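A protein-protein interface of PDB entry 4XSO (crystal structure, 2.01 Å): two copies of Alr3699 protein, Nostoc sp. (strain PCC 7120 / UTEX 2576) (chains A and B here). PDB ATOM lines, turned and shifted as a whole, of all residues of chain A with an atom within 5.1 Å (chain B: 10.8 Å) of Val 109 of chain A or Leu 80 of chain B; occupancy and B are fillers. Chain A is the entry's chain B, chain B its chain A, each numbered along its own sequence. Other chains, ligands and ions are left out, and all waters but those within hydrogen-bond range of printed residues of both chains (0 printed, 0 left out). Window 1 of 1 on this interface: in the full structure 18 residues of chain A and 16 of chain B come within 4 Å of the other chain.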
ATOM      1  N   GLN A 105      -7.694   6.298  24.647  1.00  0.00           N
ATOM      2  CA  GLN A 105      -8.513   7.179  23.789  1.00  0.00           C
ATOM      3  C   GLN A 105      -8.238   7.187  22.315  1.00  0.00           C
ATOM      4  O   GLN A 105      -9.154   7.126  21.496  1.00  0.00           O
ATOM      5  CB  GLN A 105      -8.424   8.644  24.237  1.00  0.00           C
ATOM      6  CG  GLN A 105      -9.353   9.003  25.342  1.00  0.00           C
ATOM      7  CD  GLN A 105      -9.291  10.494  25.697  1.00  0.00           C
ATOM      8  OE1 GLN A 105      -8.904  10.861  26.820  1.00  0.00           O
ATOM      9  NE2 GLN A 105      -9.648  11.353  24.737  1.00  0.00           N
ATOM     10  N   LYS A 106      -6.997   7.372  21.947  1.00  0.00           N
ATOM     11  CA  LYS A 106      -6.653   7.262  20.544  1.00  0.00           C
ATOM     12  C   LYS A 106      -6.907   5.870  19.967  1.00  0.00           C
ATOM     13  O   LYS A 106      -7.149   5.710  18.743  1.00  0.00           O
ATOM     14  CB  LYS A 106      -5.179   7.566  20.359  1.00  0.00           C
ATOM     15  CG  LYS A 106      -4.698   8.909  20.973  1.00  0.00           C
ATOM     16  CD  LYS A 106      -3.490   9.413  20.184  1.00  0.00           C
ATOM     17  CE  LYS A 106      -2.418  10.042  21.040  1.00  0.00           C
ATOM     18  NZ  LYS A 106      -2.737  11.454  21.341  1.00  0.00           N
ATOM     19  N   ALA A 107      -6.835   4.844  20.802  1.00  0.00           N
ATOM     20  CA  ALA A 107      -7.089   3.470  20.272  1.00  0.00           C
ATOM     21  C   ALA A 107      -8.566   3.375  19.996  1.00  0.00           C
ATOM     22  O   ALA A 107      -9.017   2.687  19.050  1.00  0.00           O
ATOM     23  CB  ALA A 107      -6.638   2.386  21.242  1.00  0.00           C
ATOM     24  N   LEU A 108      -9.358   4.107  20.786  1.00  0.00           N
ATOM     25  CA  LEU A 108     -10.821   4.120  20.623  1.00  0.00           C
ATOM     26  C   LEU A 108     -11.209   4.846  19.289  1.00  0.00           C
ATOM     27  O   LEU A 108     -12.038   4.393  18.503  1.00  0.00           O
ATOM     28  CB  LEU A 108     -11.554   4.732  21.867  1.00  0.00           C
ATOM     29  CG  LEU A 108     -12.985   4.992  21.389  1.00  0.00           C
ATOM     30  CD1 LEU A 108     -13.794   3.709  21.498  1.00  0.00           C
ATOM     31  CD2 LEU A 108     -13.567   6.183  22.061  1.00  0.00           C
ATOM     32  N   VAL A 109     -10.507   5.902  18.970  1.00  0.00           N
ATOM     33  CA  VAL A 109     -10.765   6.588  17.701  1.00  0.00           C
ATOM     34  C   VAL A 109     -10.471   5.707  16.495  1.00  0.00           C
ATOM     35  O   VAL A 109     -11.324   5.424  15.638  1.00  0.00           O
ATOM     36  CB  VAL A 109      -9.996   7.925  17.701  1.00  0.00           C
ATOM     37  CG1 VAL A 109     -10.115   8.596  16.366  1.00  0.00           C
ATOM     38  CG2 VAL A 109     -10.565   8.807  18.811  1.00  0.00           C
ATOM     39  N   VAL A 110      -9.257   5.193  16.463  1.00  0.00           N
ATOM     40  CA  VAL A 110      -8.863   4.306  15.401  1.00  0.00           C
ATOM     41  C   VAL A 110      -9.656   3.020  15.447  1.00  0.00           C
ATOM     42  O   VAL A 110     -10.067   2.488  14.427  1.00  0.00           O
ATOM     43  CB  VAL A 110      -7.335   4.006  15.496  1.00  0.00           C
ATOM     44  CG1 VAL A 110      -6.925   2.892  14.543  1.00  0.00           C
ATOM     45  CG2 VAL A 110      -6.518   5.264  15.293  1.00  0.00           C
ATOM     46  N   GLY A 111      -9.856   2.476  16.632  1.00  0.00           N
ATOM     47  CA  GLY A 111     -10.595   1.216  16.730  1.00  0.00           C
ATOM     48  C   GLY A 111     -12.044   1.348  16.266  1.00  0.00           C
ATOM     49  O   GLY A 111     -12.623   0.417  15.733  1.00  0.00           O
ATOM     50  N   ALA A 112     -12.644   2.515  16.495  1.00  0.00           N
ATOM     51  CA  ALA A 112     -14.034   2.798  16.034  1.00  0.00           C
ATOM     52  C   ALA A 112     -14.161   2.786  14.515  1.00  0.00           C
ATOM     53  O   ALA A 112     -15.060   2.166  13.914  1.00  0.00           O
ATOM     54  CB  ALA A 112     -14.531   4.153  16.602  1.00  0.00           C
ATOM     55  N   ILE A 113     -13.210   3.436  13.870  1.00  0.00           N
ATOM     56  CA  ILE A 113     -13.130   3.420  12.394  1.00  0.00           C
ATOM     57  C   ILE A 113     -12.905   2.028  11.888  1.00  0.00           C
ATOM     58  O   ILE A 113     -13.608   1.580  10.974  1.00  0.00           O
ATOM     59  CB  ILE A 113     -12.000   4.296  11.871  1.00  0.00           C
ATOM     60  CG1 ILE A 113     -12.322   5.724  12.240  1.00  0.00           C
ATOM     61  CG2 ILE A 113     -11.777   4.104  10.374  1.00  0.00           C
ATOM     62  CD1 ILE A 113     -11.152   6.673  12.064  1.00  0.00           C
ATOM     63  N   ASN A 139     -11.108  16.283  22.066  1.00  0.00           N
ATOM     64  CA  ASN A 139     -10.834  14.879  22.325  1.00  0.00           C
ATOM     65  C   ASN A 139     -11.994  14.234  23.073  1.00  0.00           C
ATOM     66  O   ASN A 139     -12.358  13.118  22.764  1.00  0.00           O
ATOM     67  CB  ASN A 139      -9.510  14.678  23.098  1.00  0.00           C
ATOM     68  CG  ASN A 139      -8.291  14.940  22.233  1.00  0.00           C
ATOM     69  OD1 ASN A 139      -7.490  15.872  22.461  1.00  0.00           O
ATOM     70  ND2 ASN A 139      -8.158  14.135  21.211  1.00  0.00           N
ATOM     71  N   VAL A 142     -15.100  13.743  20.734  1.00  0.00           N
ATOM     72  CA  VAL A 142     -14.811  12.741  19.729  1.00  0.00           C
ATOM     73  C   VAL A 142     -14.880  11.354  20.374  1.00  0.00           C
ATOM     74  O   VAL A 142     -15.615  10.498  19.928  1.00  0.00           O
ATOM     75  CB  VAL A 142     -13.448  13.018  19.079  1.00  0.00           C
ATOM     76  CG1 VAL A 142     -12.957  11.820  18.245  1.00  0.00           C
ATOM     77  CG2 VAL A 142     -13.595  14.210  18.148  1.00  0.00           C
ATOM     78  N   ALA A 143     -14.129  11.157  21.441  1.00  0.00           N
ATOM     79  CA  ALA A 143     -14.182   9.930  22.222  1.00  0.00           C
ATOM     80  C   ALA A 143     -15.605   9.516  22.621  1.00  0.00           C
ATOM     81  O   ALA A 143     -16.053   8.421  22.339  1.00  0.00           O
ATOM     82  CB  ALA A 143     -13.302  10.093  23.460  1.00  0.00           C
ATOM     83  N   LEU A 146     -17.806   8.635  19.411  1.00  0.00           N
ATOM     84  CA  LEU A 146     -17.441   7.400  18.765  1.00  0.00           C
ATOM     85  C   LEU A 146     -17.851   6.209  19.658  1.00  0.00           C
ATOM     86  O   LEU A 146     -18.368   5.199  19.198  1.00  0.00           O
ATOM     87  CB  LEU A 146     -15.947   7.375  18.474  1.00  0.00           C
ATOM     88  CG  LEU A 146     -15.583   8.394  17.339  1.00  0.00           C
ATOM     89  CD1 LEU A 146     -14.114   8.349  16.990  1.00  0.00           C
ATOM     90  CD2 LEU A 146     -16.342   8.021  16.092  1.00  0.00           C
ATOM     91  N   PRO B  64       2.043  15.564   8.060  1.00  0.00           N
ATOM     92  CA  PRO B  64       1.802  15.812   9.492  1.00  0.00           C
ATOM     93  C   PRO B  64       1.282  17.212   9.794  1.00  0.00           C
ATOM     94  O   PRO B  64       1.623  18.121   9.062  1.00  0.00           O
ATOM     95  CB  PRO B  64       3.189  15.577  10.104  1.00  0.00           C
ATOM     96  CG  PRO B  64       3.731  14.447   9.263  1.00  0.00           C
ATOM     97  CD  PRO B  64       3.275  14.765   7.856  1.00  0.00           C
ATOM     98  N   SER B  79      -6.160  18.079  18.836  1.00  0.00           N
ATOM     99  CA  SER B  79      -6.900  17.736  17.627  1.00  0.00           C
ATOM    100  C   SER B  79      -7.036  16.224  17.474  1.00  0.00           C
ATOM    101  O   SER B  79      -8.041  15.731  16.962  1.00  0.00           O
ATOM    102  CB  SER B  79      -6.216  18.330  16.395  1.00  0.00           C
ATOM    103  OG  SER B  79      -7.153  18.577  15.360  1.00  0.00           O
ATOM    104  N   LEU B  80      -6.020  15.496  17.922  1.00  0.00           N
ATOM    105  CA  LEU B  80      -6.024  14.040  17.836  1.00  0.00           C
ATOM    106  C   LEU B  80      -5.723  13.570  16.417  1.00  0.00           C
ATOM    107  O   LEU B  80      -5.872  12.389  16.099  1.00  0.00           O
ATOM    108  CB  LEU B  80      -7.368  13.480  18.302  1.00  0.00           C
ATOM    109  CG  LEU B  80      -7.521  11.959  18.256  1.00  0.00           C
ATOM    110  CD1 LEU B  80      -7.980  11.423  19.604  1.00  0.00           C
ATOM    111  CD2 LEU B  80      -8.486  11.547  17.154  1.00  0.00           C
ATOM    112  N   GLY B  81      -5.300  14.499  15.568  1.00  0.00           N
ATOM    113  CA  GLY B  81      -4.979  14.183  14.187  1.00  0.00           C
ATOM    114  C   GLY B  81      -3.634  13.678  13.701  1.00  0.00           C
ATOM    115  O   GLY B  81      -3.458  13.493  12.518  1.00  0.00           O
ATOM    116  N   GLN B  82      -2.685  13.443  14.591  1.00  0.00           N
ATOM    117  CA  GLN B  82      -1.405  12.826  14.228  1.00  0.00           C
ATOM    118  C   GLN B  82      -1.620  11.423  13.679  1.00  0.00           C
ATOM    119  O   GLN B  82      -0.860  10.938  12.868  1.00  0.00           O
ATOM    120  CB  GLN B  82      -0.478  12.748  15.442  1.00  0.00           C
ATOM    121  CG  GLN B  82       0.615  13.807  15.535  1.00  0.00           C
ATOM    122  CD  GLN B  82       1.402  14.024  14.244  1.00  0.00           C
ATOM    123  OE1 GLN B  82       1.929  13.086  13.642  1.00  0.00           O
ATOM    124  NE2 GLN B  82       1.496  15.285  13.825  1.00  0.00           N
ATOM    125  N   LEU B  83      -2.650  10.770  14.180  1.00  0.00           N
ATOM    126  CA  LEU B  83      -2.979   9.425  13.778  1.00  0.00           C
ATOM    127  C   LEU B  83      -3.325   9.304  12.302  1.00  0.00           C
ATOM    128  O   LEU B  83      -2.931   8.353  11.669  1.00  0.00           O
ATOM    129  CB  LEU B  83      -4.147   8.924  14.595  1.00  0.00           C
ATOM    130  CG  LEU B  83      -4.069   8.996  16.108  1.00  0.00           C
ATOM    131  CD1 LEU B  83      -5.437   9.213  16.703  1.00  0.00           C
ATOM    132  CD2 LEU B  83      -3.486   7.713  16.638  1.00  0.00           C
ATOM    133  N   ALA B  84      -4.063  10.271  11.762  1.00  0.00           N
ATOM    134  CA  ALA B  84      -4.602  10.190  10.361  1.00  0.00           C
ATOM    135  C   ALA B  84      -4.701  11.598   9.772  1.00  0.00           C
ATOM    136  O   ALA B  84      -5.778  12.167   9.806  1.00  0.00           O
ATOM    137  CB  ALA B  84      -6.003   9.553  10.387  1.00  0.00           C
ATOM    138  N   PRO B  85      -3.556  12.188   9.346  1.00  0.00           N
ATOM    139  CA  PRO B  85      -3.543  13.653   9.156  1.00  0.00           C
ATOM    140  C   PRO B  85      -4.515  14.146   8.053  1.00  0.00           C
ATOM    141  O   PRO B  85      -5.179  15.139   8.249  1.00  0.00           O
ATOM    142  CB  PRO B  85      -2.075  13.955   8.819  1.00  0.00           C
ATOM    143  CG  PRO B  85      -1.310  12.824   9.490  1.00  0.00           C
ATOM    144  CD  PRO B  85      -2.189  11.613   9.345  1.00  0.00           C
ATOM    145  N   LEU B  86      -4.580  13.438   6.940  1.00  0.00           N
ATOM    146  CA  LEU B  86      -5.582  13.754   5.915  1.00  0.00           C
ATOM    147  C   LEU B  86      -6.965  13.808   6.555  1.00  0.00           C
ATOM    148  O   LEU B  86      -7.662  14.837   6.458  1.00  0.00           O
ATOM    149  CB  LEU B  86      -5.544  12.780   4.753  1.00  0.00           C
ATOM    150  CG  LEU B  86      -6.568  12.967   3.585  1.00  0.00           C
ATOM    151  CD1 LEU B  86      -6.722  14.401   3.146  1.00  0.00           C
ATOM    152  CD2 LEU B  86      -6.101  12.188   2.368  1.00  0.00           C
ATOM    153  N   VAL B  87      -7.354  12.733   7.247  1.00  0.00           N
ATOM    154  CA  VAL B  87      -8.709  12.661   7.806  1.00  0.00           C
ATOM    155  C   VAL B  87      -8.927  13.800   8.819  1.00  0.00           C
ATOM    156  O   VAL B  87      -9.942  14.489   8.802  1.00  0.00           O
ATOM    157  CB  VAL B  87      -8.908  11.277   8.438  1.00  0.00           C
ATOM    158  CG1 VAL B  87     -10.194  11.205   9.219  1.00  0.00           C
ATOM    159  CG2 VAL B  87      -8.756  10.184   7.371  1.00  0.00           C
ATOM    160  N   ALA B  88      -7.914  14.101   9.634  1.00  0.00           N
ATOM    161  CA  ALA B  88      -8.051  15.162  10.649  1.00  0.00           C
ATOM    162  C   ALA B  88      -8.275  16.508  10.033  1.00  0.00           C
ATOM    163  O   ALA B  88      -8.998  17.364  10.584  1.00  0.00           O
ATOM    164  CB  ALA B  88      -6.815  15.241  11.517  1.00  0.00           C
ATOM    165  N   LYS B  89      -7.623  16.754   8.911  1.00  0.00           N
ATOM    166  CA  LYS B  89      -7.821  18.091   8.299  1.00  0.00           C
ATOM    167  C   LYS B  89      -9.264  18.170   7.712  1.00  0.00           C
ATOM    168  O   LYS B  89      -9.959  19.174   7.907  1.00  0.00           O
ATOM    169  CB  LYS B  89      -6.761  18.337   7.235  1.00  0.00           C
ATOM    170  CG  LYS B  89      -5.311  18.385   7.729  1.00  0.00           C
ATOM    171  CD  LYS B  89      -4.345  18.010   6.612  1.00  0.00           C
ATOM    172  CE  LYS B  89      -2.890  18.091   7.074  1.00  0.00           C
ATOM    173  NZ  LYS B  89      -1.945  17.559   6.043  1.00  0.00           N
ATOM    174  N   VAL B  90      -9.713  17.079   7.079  1.00  0.00           N
ATOM    175  CA  VAL B  90     -11.028  17.064   6.451  1.00  0.00           C
ATOM    176  C   VAL B  90     -11.987  17.244   7.591  1.00  0.00           C
ATOM    177  O   VAL B  90     -12.813  18.133   7.534  1.00  0.00           O
ATOM    178  CB  VAL B  90     -11.292  15.787   5.622  1.00  0.00           C
ATOM    179  CG1 VAL B  90     -12.725  15.741   5.092  1.00  0.00           C
ATOM    180  CG2 VAL B  90     -10.352  15.719   4.449  1.00  0.00           C
ATOM    181  N   VAL B  91     -11.837  16.451   8.671  1.00  0.00           N
ATOM    182  CA  VAL B  91     -12.742  16.570   9.832  1.00  0.00           C
ATOM    183  C   VAL B  91     -12.779  17.957  10.361  1.00  0.00           C
ATOM    184  O   VAL B  91     -13.831  18.486  10.610  1.00  0.00           O
ATOM    185  CB  VAL B  91     -12.368  15.619  11.015  1.00  0.00           C
ATOM    186  CG1 VAL B  91     -13.198  15.961  12.235  1.00  0.00           C
ATOM    187  CG2 VAL B  91     -12.550  14.155  10.643  1.00  0.00           C
ATOM    188  N   GLN B  92     -11.625  18.580  10.534  1.00  0.00           N
ATOM    189  CA  GLN B  92     -11.601  19.945  11.069  1.00  0.00           C
ATOM    190  C   GLN B  92     -12.207  20.989  10.122  1.00  0.00           C
ATOM    191  O   GLN B  92     -12.874  21.906  10.548  1.00  0.00           O
ATOM    192  CB  GLN B  92     -10.168  20.394  11.367  1.00  0.00           C
ATOM    193  CG  GLN B  92     -10.124  21.798  11.960  1.00  0.00           C
ATOM    194  CD  GLN B  92      -8.831  22.511  11.649  1.00  0.00           C
ATOM    195  OE1 GLN B  92      -7.756  21.899  11.631  1.00  0.00           O
ATOM    196  NE2 GLN B  92      -8.918  23.815  11.410  1.00  0.00           N
ATOM    197  N   ILE B 113     -15.991   8.946   7.135  1.00  0.00           N
ATOM    198  CA  ILE B 113     -15.266   9.091   8.415  1.00  0.00           C
ATOM    199  C   ILE B 113     -15.391  10.463   8.995  1.00  0.00           C
ATOM    200  O   ILE B 113     -15.798  10.658  10.161  1.00  0.00           O
ATOM    201  CB  ILE B 113     -13.777   8.702   8.259  1.00  0.00           C
ATOM    202  CG1 ILE B 113     -13.680   7.267   7.737  1.00  0.00           C
ATOM    203  CG2 ILE B 113     -13.078   8.841   9.564  1.00  0.00           C
ATOM    204  CD1 ILE B 113     -12.286   6.866   7.241  1.00  0.00           C
ATOM    205  N   ALA B 114     -15.119  11.457   8.191  1.00  0.00           N
ATOM    206  CA  ALA B 114     -15.357  12.814   8.645  1.00  0.00           C
ATOM    207  C   ALA B 114     -16.783  13.097   8.961  1.00  0.00           C
ATOM    208  O   ALA B 114     -17.095  13.958   9.838  1.00  0.00           O
ATOM    209  CB  ALA B 114     -14.892  13.805   7.579  1.00  0.00           C
ATOM    210  N   PHE B 116     -19.035  11.107  10.289  1.00  0.00           N
ATOM    211  CA  PHE B 116     -19.330  10.700  11.638  1.00  0.00           C
ATOM    212  C   PHE B 116     -18.600  11.452  12.747  1.00  0.00           C
ATOM    213  O   PHE B 116     -19.235  11.956  13.629  1.00  0.00           O
ATOM    214  CB  PHE B 116     -19.524   9.185  11.849  1.00  0.00           C
ATOM    215  CG  PHE B 116     -18.352   8.303  11.517  1.00  0.00           C
ATOM    216  CD1 PHE B 116     -17.283   8.181  12.375  1.00  0.00           C
ATOM    217  CD2 PHE B 116     -18.388   7.487  10.417  1.00  0.00           C
ATOM    218  CE1 PHE B 116     -16.244   7.322  12.105  1.00  0.00           C
ATOM    219  CE2 PHE B 116     -17.352   6.623  10.137  1.00  0.00           C
ATOM    220  CZ  PHE B 116     -16.276   6.534  10.989  1.00  0.00           C
ATOM    221  N   ILE B 117     -17.311  11.663  12.604  1.00  0.00           N
ATOM    222  CA  ILE B 117     -16.544  12.413  13.599  1.00  0.00           C
ATOM    223  C   ILE B 117     -17.006  13.861  13.717  1.00  0.00           C
ATOM    224  O   ILE B 117     -17.150  14.325  14.796  1.00  0.00           O
ATOM    225  CB  ILE B 117     -15.031  12.336  13.387  1.00  0.00           C
ATOM    226  CG1 ILE B 117     -14.564  10.903  13.500  1.00  0.00           C
ATOM    227  CG2 ILE B 117     -14.302  13.270  14.363  1.00  0.00           C
ATOM    228  CD1 ILE B 117     -13.198  10.682  12.904  1.00  0.00           C
ATOM    229  N   ALA B 118     -17.246  14.590  12.636  1.00  0.00           N
ATOM    230  CA  ALA B 118     -17.651  15.994  12.767  1.00  0.00           C
ATOM    231  C   ALA B 118     -19.158  16.213  12.851  1.00  0.00           C
ATOM    232  O   ALA B 118     -19.616  17.338  12.990  1.00  0.00           O
ATOM    233  CB  ALA B 118     -17.102  16.813  11.600  1.00  0.00           C
ATOM    234  N   PHE B 150     -23.544   5.624   6.277  1.00  0.00           N
ATOM    235  CA  PHE B 150     -23.317   7.042   6.613  1.00  0.00           C
ATOM    236  C   PHE B 150     -23.914   8.035   5.642  1.00  0.00           C
ATOM    237  O   PHE B 150     -24.102   9.208   5.977  1.00  0.00           O
ATOM    238  CB  PHE B 150     -21.823   7.332   6.751  1.00  0.00           C
ATOM    239  CG  PHE B 150     -21.203   6.567   7.827  1.00  0.00           C
ATOM    240  CD1 PHE B 150     -21.514   6.873   9.123  1.00  0.00           C
ATOM    241  CD2 PHE B 150     -20.475   5.401   7.557  1.00  0.00           C
ATOM    242  CE1 PHE B 150     -21.041   6.075  10.176  1.00  0.00           C
ATOM    243  CE2 PHE B 150     -19.950   4.610   8.618  1.00  0.00           C
ATOM    244  CZ  PHE B 150     -20.268   4.935   9.919  1.00  0.00           C
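Among the printed residues, pairs that only touch across the chains: Asn 139 of chain A with Leu 80 of chain B (3.1 Å), Val 109 of chain A with Leu 80 of chain B (3.5 Å), Ile 113 of chain A with Ile 113 of chain B (3.8 Å), Leu 146 of chain A with Phe 116 of chain B (3.8 Å), Lys 106 of chain A with Leu 83 of chain B (3.9 Å) and Val 142 of chain A with Ile 117 of chain B (3.96 Å).
Of the 13 printed residues of chain A, 6 touch a printed residue of chain B. Hydrophobic or aromatic side chains of chain A within 4 Å of the printed part of chain B: Val 109, Ile 113, Val 142 and Leu 146. Hydrophobic or aromatic side chains of chain B within 4 Å of the printed part of chain A: Leu 80, Leu 83, Ile 113, Phe 116 and Ile 117. Among the printed residues, 6 pairs touch across the chains. Among the printed residues, no Asp or Glu carboxylate lies within 4 Å of a Lys or Arg side-chain nitrogen of the other chain.
Leu 80 of chain B touches two residues of chain A. Lys 106 of chain A touches just one residue of chain B: Leu 83. Ala 107 of chain A touches none of the printed residues of chain B. No residue of chain B comes within 4 Å of Leu 108 of chain A. No residue of chain B comes within 4 Å of Val 110 of chain A. Ala 112 of chain A touches none of the printed residues of chain B. Ile 113 of chain A touches just one residue of chain B: Ile 113. No residue of chain B comes within 4 Å of Ala 143 of chain A. Of the printed residues of chain B, Val 142 of chain A touches Ile 117. Of the printed residues of chain A, Phe 116 of chain B touches Leu 146. Ala 84 of chain B touches none of the printed residues of chain A. Gln 92 of chain B touches none of the printed residues of chain A. The nearest residue of chain A that does not touch Leu 80 of chain B is Lys 106 of chain A (4.4 Å). The nearest printed residue of chain A that does not touch Ile 117 of chain B is Leu 146 of chain A (4.3 Å).
Ile 113 of chain B touches its own counterpart, Ile 113 of chain A. Position printed for both chains: 113. Of the 6 pairs that touch across the chains among the printed residues, 1 has its exchanged pair printed and touching as well.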
